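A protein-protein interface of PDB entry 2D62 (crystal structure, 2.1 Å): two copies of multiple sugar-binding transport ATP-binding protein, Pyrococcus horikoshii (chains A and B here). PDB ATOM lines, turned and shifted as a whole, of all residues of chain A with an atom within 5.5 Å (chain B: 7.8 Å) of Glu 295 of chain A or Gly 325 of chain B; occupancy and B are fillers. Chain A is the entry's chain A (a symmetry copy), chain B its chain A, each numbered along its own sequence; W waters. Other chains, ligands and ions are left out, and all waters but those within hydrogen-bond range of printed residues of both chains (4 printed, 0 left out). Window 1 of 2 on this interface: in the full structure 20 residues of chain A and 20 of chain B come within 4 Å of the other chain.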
ATOM      1  N   TYR A 231      22.962   6.391  12.394  1.00  0.00           N
ATOM      2  CA  TYR A 231      22.129   6.604  13.571  1.00  0.00           C
ATOM      3  C   TYR A 231      21.737   5.279  14.240  1.00  0.00           C
ATOM      4  O   TYR A 231      21.897   5.119  15.449  1.00  0.00           O
ATOM      5  CB  TYR A 231      20.863   7.380  13.194  1.00  0.00           C
ATOM      6  CG  TYR A 231      20.000   7.760  14.379  1.00  0.00           C
ATOM      7  CD1 TYR A 231      20.267   8.910  15.119  1.00  0.00           C
ATOM      8  CD2 TYR A 231      18.921   6.965  14.766  1.00  0.00           C
ATOM      9  CE1 TYR A 231      19.481   9.265  16.211  1.00  0.00           C
ATOM     10  CE2 TYR A 231      18.123   7.311  15.865  1.00  0.00           C
ATOM     11  CZ  TYR A 231      18.412   8.463  16.580  1.00  0.00           C
ATOM     12  OH  TYR A 231      17.643   8.822  17.665  1.00  0.00           O
ATOM     13  N   TYR A 232      21.242   4.332  13.447  1.00  0.00           N
ATOM     14  CA  TYR A 232      20.810   3.031  13.969  1.00  0.00           C
ATOM     15  C   TYR A 232      21.884   1.960  14.066  1.00  0.00           C
ATOM     16  O   TYR A 232      21.769   1.044  14.881  1.00  0.00           O
ATOM     17  CB  TYR A 232      19.667   2.478  13.117  1.00  0.00           C
ATOM     18  CG  TYR A 232      18.421   3.318  13.169  1.00  0.00           C
ATOM     19  CD1 TYR A 232      17.667   3.400  14.339  1.00  0.00           C
ATOM     20  CD2 TYR A 232      17.997   4.042  12.056  1.00  0.00           C
ATOM     21  CE1 TYR A 232      16.518   4.181  14.400  1.00  0.00           C
ATOM     22  CE2 TYR A 232      16.850   4.829  12.105  1.00  0.00           C
ATOM     23  CZ  TYR A 232      16.117   4.892  13.284  1.00  0.00           C
ATOM     24  OH  TYR A 232      14.984   5.663  13.354  1.00  0.00           O
ATOM     25  N   ARG A 293      19.635   4.202  23.400  1.00  0.00           N
ATOM     26  CA  ARG A 293      19.280   5.609  23.347  1.00  0.00           C
ATOM     27  C   ARG A 293      18.159   5.901  24.333  1.00  0.00           C
ATOM     28  O   ARG A 293      17.299   5.056  24.577  1.00  0.00           O
ATOM     29  CB  ARG A 293      18.832   6.003  21.939  1.00  0.00           C
ATOM     30  CG  ARG A 293      19.948   5.973  20.898  1.00  0.00           C
ATOM     31  CD  ARG A 293      19.483   6.541  19.560  1.00  0.00           C
ATOM     32  NE  ARG A 293      20.530   6.440  18.544  1.00  0.00           N
ATOM     33  CZ  ARG A 293      21.622   7.197  18.512  1.00  0.00           C
ATOM     34  NH1 ARG A 293      21.825   8.130  19.439  1.00  0.00           N
ATOM     35  NH2 ARG A 293      22.529   7.005  17.566  1.00  0.00           N
ATOM     36  N   PRO A 294      18.175   7.098  24.937  1.00  0.00           N
ATOM     37  CA  PRO A 294      17.140   7.490  25.896  1.00  0.00           C
ATOM     38  C   PRO A 294      15.731   7.301  25.327  1.00  0.00           C
ATOM     39  O   PRO A 294      14.801   6.960  26.056  1.00  0.00           O
ATOM     40  CB  PRO A 294      17.465   8.956  26.160  1.00  0.00           C
ATOM     41  CG  PRO A 294      18.968   8.953  26.134  1.00  0.00           C
ATOM     42  CD  PRO A 294      19.278   8.076  24.919  1.00  0.00           C
ATOM     43  N   GLU A 295      15.578   7.510  24.022  1.00  0.00           N
ATOM     44  CA  GLU A 295      14.263   7.372  23.403  1.00  0.00           C
ATOM     45  C   GLU A 295      13.765   5.931  23.449  1.00  0.00           C
ATOM     46  O   GLU A 295      12.580   5.672  23.237  1.00  0.00           O
ATOM     47  CB  GLU A 295      14.300   7.865  21.949  1.00  0.00           C
ATOM     48  CG  GLU A 295      15.016   6.940  20.967  1.00  0.00           C
ATOM     49  CD  GLU A 295      15.298   7.615  19.632  1.00  0.00           C
ATOM     50  OE1 GLU A 295      14.641   8.630  19.327  1.00  0.00           O
ATOM     51  OE2 GLU A 295      16.171   7.130  18.882  1.00  0.00           O
ATOM     52  N   ASP A 296      14.665   4.993  23.726  1.00  0.00           N
ATOM     53  CA  ASP A 296      14.275   3.589  23.785  1.00  0.00           C
ATOM     54  C   ASP A 296      14.143   3.056  25.207  1.00  0.00           C
ATOM     55  O   ASP A 296      14.007   1.853  25.422  1.00  0.00           O
ATOM     56  CB  ASP A 296      15.243   2.740  22.959  1.00  0.00           C
ATOM     57  CG  ASP A 296      15.214   3.113  21.487  1.00  0.00           C
ATOM     58  OD1 ASP A 296      14.109   3.122  20.900  1.00  0.00           O
ATOM     59  OD2 ASP A 296      16.289   3.402  20.918  1.00  0.00           O
ATOM     60  N   VAL A 297      14.198   3.967  26.174  1.00  0.00           N
ATOM     61  CA  VAL A 297      14.003   3.626  27.577  1.00  0.00           C
ATOM     62  C   VAL A 297      12.677   4.326  27.866  1.00  0.00           C
ATOM     63  O   VAL A 297      12.590   5.561  27.829  1.00  0.00           O
ATOM     64  CB  VAL A 297      15.102   4.200  28.489  1.00  0.00           C
ATOM     65  CG1 VAL A 297      14.807   3.821  29.944  1.00  0.00           C
ATOM     66  CG2 VAL A 297      16.470   3.655  28.073  1.00  0.00           C
ATOM     67  N   HIS A 298      11.647   3.534  28.139  1.00  0.00           N
ATOM     68  CA  HIS A 298      10.309   4.061  28.359  1.00  0.00           C
ATOM     69  C   HIS A 298       9.766   4.025  29.778  1.00  0.00           C
ATOM     70  O   HIS A 298      10.129   3.170  30.588  1.00  0.00           O
ATOM     71  CB  HIS A 298       9.318   3.301  27.474  1.00  0.00           C
ATOM     72  CG  HIS A 298       9.670   3.304  26.021  1.00  0.00           C
ATOM     73  ND1 HIS A 298       9.115   4.190  25.122  1.00  0.00           N
ATOM     74  CD2 HIS A 298      10.520   2.526  25.307  1.00  0.00           C
ATOM     75  CE1 HIS A 298       9.606   3.955  23.917  1.00  0.00           C
ATOM     76  NE2 HIS A 298      10.461   2.951  24.002  1.00  0.00           N
ATOM     77  N   ALA A 340      16.326   8.513  30.168  1.00  0.00           N
ATOM     78  CA  ALA A 340      15.176   8.055  29.402  1.00  0.00           C
ATOM     79  C   ALA A 340      14.352   9.250  28.954  1.00  0.00           C
ATOM     80  O   ALA A 340      14.502  10.350  29.483  1.00  0.00           O
ATOM     81  CB  ALA A 340      14.310   7.133  30.258  1.00  0.00           C
ATOM     82  N   LYS A 341      13.493   9.037  27.964  1.00  0.00           N
ATOM     83  CA  LYS A 341      12.605  10.093  27.503  1.00  0.00           C
ATOM     84  C   LYS A 341      11.206   9.718  27.964  1.00  0.00           C
ATOM     85  O   LYS A 341      10.731   8.614  27.683  1.00  0.00           O
ATOM     86  CB  LYS A 341      12.613  10.217  25.978  1.00  0.00           C
ATOM     87  CG  LYS A 341      13.819  10.925  25.401  1.00  0.00           C
ATOM     88  CD  LYS A 341      13.548  11.291  23.949  1.00  0.00           C
ATOM     89  CE  LYS A 341      14.666  12.121  23.354  1.00  0.00           C
ATOM     90  NZ  LYS A 341      14.301  12.573  21.982  1.00  0.00           N
ATOM     91  N   ASN B 322      15.672  16.169   9.500  1.00  0.00           N
ATOM     92  CA  ASN B 322      15.944  14.895  10.142  1.00  0.00           C
ATOM     93  C   ASN B 322      16.705  15.180  11.427  1.00  0.00           C
ATOM     94  O   ASN B 322      17.909  15.411  11.398  1.00  0.00           O
ATOM     95  CB  ASN B 322      16.786  14.008   9.231  1.00  0.00           C
ATOM     96  CG  ASN B 322      16.952  12.609   9.784  1.00  0.00           C
ATOM     97  OD1 ASN B 322      16.613  12.349  10.932  1.00  0.00           O
ATOM     98  ND2 ASN B 322      17.483  11.701   8.970  1.00  0.00           N
ATOM     99  N   LEU B 323      15.998  15.172  12.554  1.00  0.00           N
ATOM    100  CA  LEU B 323      16.629  15.442  13.837  1.00  0.00           C
ATOM    101  C   LEU B 323      17.087  14.152  14.504  1.00  0.00           C
ATOM    102  O   LEU B 323      17.503  14.161  15.658  1.00  0.00           O
ATOM    103  CB  LEU B 323      15.663  16.183  14.766  1.00  0.00           C
ATOM    104  CG  LEU B 323      14.912  17.401  14.218  1.00  0.00           C
ATOM    105  CD1 LEU B 323      14.188  18.088  15.378  1.00  0.00           C
ATOM    106  CD2 LEU B 323      15.866  18.374  13.547  1.00  0.00           C
ATOM    107  N   GLY B 324      17.006  13.044  13.780  1.00  0.00           N
ATOM    108  CA  GLY B 324      17.436  11.776  14.342  1.00  0.00           C
ATOM    109  C   GLY B 324      16.332  11.046  15.083  1.00  0.00           C
ATOM    110  O   GLY B 324      15.874   9.992  14.637  1.00  0.00           O
ATOM    111  N   GLY B 325      15.903  11.600  16.214  1.00  0.00           N
ATOM    112  CA  GLY B 325      14.844  10.973  16.989  1.00  0.00           C
ATOM    113  C   GLY B 325      13.452  11.272  16.456  1.00  0.00           C
ATOM    114  O   GLY B 325      12.460  10.703  16.916  1.00  0.00           O
ATOM    115  N   GLU B 326      13.376  12.165  15.474  1.00  0.00           N
ATOM    116  CA  GLU B 326      12.105  12.556  14.874  1.00  0.00           C
ATOM    117  C   GLU B 326      12.351  13.383  13.620  1.00  0.00           C
ATOM    118  O   GLU B 326      13.471  13.813  13.361  1.00  0.00           O
ATOM    119  CB  GLU B 326      11.285  13.389  15.866  1.00  0.00           C
ATOM    120  CG  GLU B 326      12.059  14.561  16.464  1.00  0.00           C
ATOM    121  CD  GLU B 326      11.185  15.498  17.285  1.00  0.00           C
ATOM    122  OE1 GLU B 326      10.225  15.019  17.929  1.00  0.00           O
ATOM    123  OE2 GLU B 326      11.466  16.718  17.300  1.00  0.00           O
ATOM    124  N   LYS B 327      11.293  13.603  12.850  1.00  0.00           N
ATOM    125  CA  LYS B 327      11.375  14.397  11.635  1.00  0.00           C
ATOM    126  C   LYS B 327      10.431  15.586  11.737  1.00  0.00           C
ATOM    127  O   LYS B 327       9.279  15.437  12.140  1.00  0.00           O
ATOM    128  CB  LYS B 327      10.986  13.553  10.418  1.00  0.00           C
ATOM    129  CG  LYS B 327      12.019  12.517   9.999  1.00  0.00           C
ATOM    130  CD  LYS B 327      11.480  11.640   8.875  1.00  0.00           C
ATOM    131  CE  LYS B 327      12.564  10.733   8.292  1.00  0.00           C
ATOM    132  NZ  LYS B 327      13.247   9.921   9.327  1.00  0.00           N
ATOM    133  N   PHE B 342       6.734  14.255  12.454  1.00  0.00           N
ATOM    134  CA  PHE B 342       6.512  12.892  11.985  1.00  0.00           C
ATOM    135  C   PHE B 342       7.475  11.961  12.715  1.00  0.00           C
ATOM    136  O   PHE B 342       8.593  12.356  13.061  1.00  0.00           O
ATOM    137  CB  PHE B 342       6.785  12.768  10.482  1.00  0.00           C
ATOM    138  CG  PHE B 342       5.635  13.182   9.595  1.00  0.00           C
ATOM    139  CD1 PHE B 342       5.559  12.706   8.284  1.00  0.00           C
ATOM    140  CD2 PHE B 342       4.659  14.066  10.042  1.00  0.00           C
ATOM    141  CE1 PHE B 342       4.531  13.105   7.432  1.00  0.00           C
ATOM    142  CE2 PHE B 342       3.628  14.472   9.198  1.00  0.00           C
ATOM    143  CZ  PHE B 342       3.564  13.991   7.889  1.00  0.00           C
ATOM    144  N   PRO B 343       7.059  10.711  12.960  1.00  0.00           N
ATOM    145  CA  PRO B 343       7.967   9.796  13.650  1.00  0.00           C
ATOM    146  C   PRO B 343       9.185   9.531  12.768  1.00  0.00           C
ATOM    147  O   PRO B 343       9.127   9.701  11.549  1.00  0.00           O
ATOM    148  CB  PRO B 343       7.106   8.553  13.878  1.00  0.00           C
ATOM    149  CG  PRO B 343       6.118   8.605  12.752  1.00  0.00           C
ATOM    150  CD  PRO B 343       5.762  10.071  12.688  1.00  0.00           C
ATOM    151  N   LYS B 344      10.291   9.134  13.386  1.00  0.00           N
ATOM    152  CA  LYS B 344      11.515   8.872  12.637  1.00  0.00           C
ATOM    153  C   LYS B 344      11.369   7.725  11.635  1.00  0.00           C
ATOM    154  O   LYS B 344      12.064   7.697  10.619  1.00  0.00           O
ATOM    155  CB  LYS B 344      12.676   8.590  13.601  1.00  0.00           C
ATOM    156  CG  LYS B 344      12.453   7.427  14.564  1.00  0.00           C
ATOM    157  CD  LYS B 344      13.620   7.319  15.541  1.00  0.00           C
ATOM    158  CE  LYS B 344      13.532   6.070  16.403  1.00  0.00           C
ATOM    159  NZ  LYS B 344      12.334   6.078  17.282  1.00  0.00           N
ATOM    160  N   GLU B 345      10.460   6.793  11.902  1.00  0.00           N
ATOM    161  CA  GLU B 345      10.265   5.667  10.992  1.00  0.00           C
ATOM    162  C   GLU B 345       9.412   5.995   9.768  1.00  0.00           C
ATOM    163  O   GLU B 345       9.144   5.123   8.940  1.00  0.00           O
ATOM    164  CB  GLU B 345       9.673   4.464  11.738  1.00  0.00           C
ATOM    165  CG  GLU B 345       8.753   4.822  12.881  1.00  0.00           C
ATOM    166  CD  GLU B 345       9.505   5.278  14.119  1.00  0.00           C
ATOM    167  OE1 GLU B 345       9.098   6.295  14.709  1.00  0.00           O
ATOM    168  OE2 GLU B 345      10.491   4.616  14.511  1.00  0.00           O
HETATM  169  O   HOH W   1      14.735   7.185  10.779  1.00  0.00           O
HETATM  170  O   HOH W   2      11.776   8.208  18.733  1.00  0.00           O
HETATM  171  O   HOH W   3      13.519   3.674  18.356  1.00  0.00           O
HETATM  172  O   HOH W   4      12.564  10.552  20.068  1.00  0.00           O
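NZ of Lys 327 of chain B lies within hydrogen-bond range of O of Lys 344 of chain B (2.8 Å).
NZ of Lys 344 of chain B lies within salt-bridge range of OE2 of Glu 345 of chain B (3.6 Å).
The side-chain amide oxygen of Asn 322 of chain B lies within hydrogen-bond range of the backbone NH of Gly 324 of chain B (3.0 Å).
O of Tyr 231 of chain A lies within hydrogen-bond range of NH2 of Arg 293 of chain A, 2.9 Å away.
The side-chain hydroxyl (OH) of Tyr 231 of chain A lies within hydrogen-bond range of the side-chain carboxylate (OE2) of Glu 295 of chain A, 2.6 Å away.
No position is printed for both chains.
CZ of Tyr 231 of chain A touches O of Gly 324 of chain B, at 3.5 Å.
Gly 325 of chain B touches Tyr 231 of chain A (N to OH, 3.6 Å).
Tyr 232 of chain A touches Lys 344 of chain B.
Glu 295 of chain A touches Gly 325 of chain B (OE1 to CA, 3.3 Å).
Lys 344 of chain B touches Glu 295 of chain A.
Of the 10 printed residues of chain A, 3 touch a printed residue of chain B.
Hydrophobic or aromatic side chains of chain A that line the printed part of chain B: Tyr 231 and Tyr 232.
Along chain A the printed residues that touch a printed residue of chain B span positions 231 to 295.
Of the 10 printed residues of chain B, 3 touch a printed residue of chain A.
Printed residues of chain B that touch a printed residue of chain A: Gly 324, Gly 325 and Lys 344.
Among the printed residues, no Asp or Glu carboxylate lies within 4 Å of a Lys or Arg side-chain nitrogen of the other chain.
Glu 295 of chain A touches two residues of chain B.
Printed residues of chain A within 4 Å of Gly 325 of chain B: Tyr 231 and Glu 295.
Printed residues of chain B within 4 Å of Tyr 232 of chain A: Lys 344 (3.1 Å).
Of the printed residues of chain A, Lys 344 of chain B touches Tyr 232 and Glu 295.
Printed residues of chain B within 4 Å of Tyr 231 of chain A: Gly 324 and Gly 325.
Printed residues of chain A within 4 Å of Gly 324 of chain B: Tyr 231.
Asn 322 of chain B touches none of the printed residues of chain A.
The nearest residue of chain B that does not touch Glu 295 of chain A is Gly 324 of chain B (5.0 Å).
The nearest residue of chain A that does not touch Gly 325 of chain B is Lys 341 of chain A (5.3 Å).
The nearest printed residue of chain B that does not touch Tyr 232 of chain A is Gly 324 of chain B (4.6 Å).
Water W2 lies within hydrogen-bond range of the side-chain amino group of Lys 344 of chain B, the side-chain carboxylate of Glu 295 of chain A and the backbone carbonyl oxygen of Gly 325 of chain B.
Water W3 bridges OD1 of Asp 296 of chain A and NZ of Lys 344 of chain B.
Water W1 lies within hydrogen-bond range of O of Lys 344 of chain B, OH of Tyr 232 of chain A and NZ of Lys 327 of chain B.
Water W4 lies within hydrogen-bond range of OE1 of Glu 295 of chain A (2.9 Å), O of Gly 325 of chain B (3.2 Å) and NZ of Lys 341 of chain A (3.3 Å).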
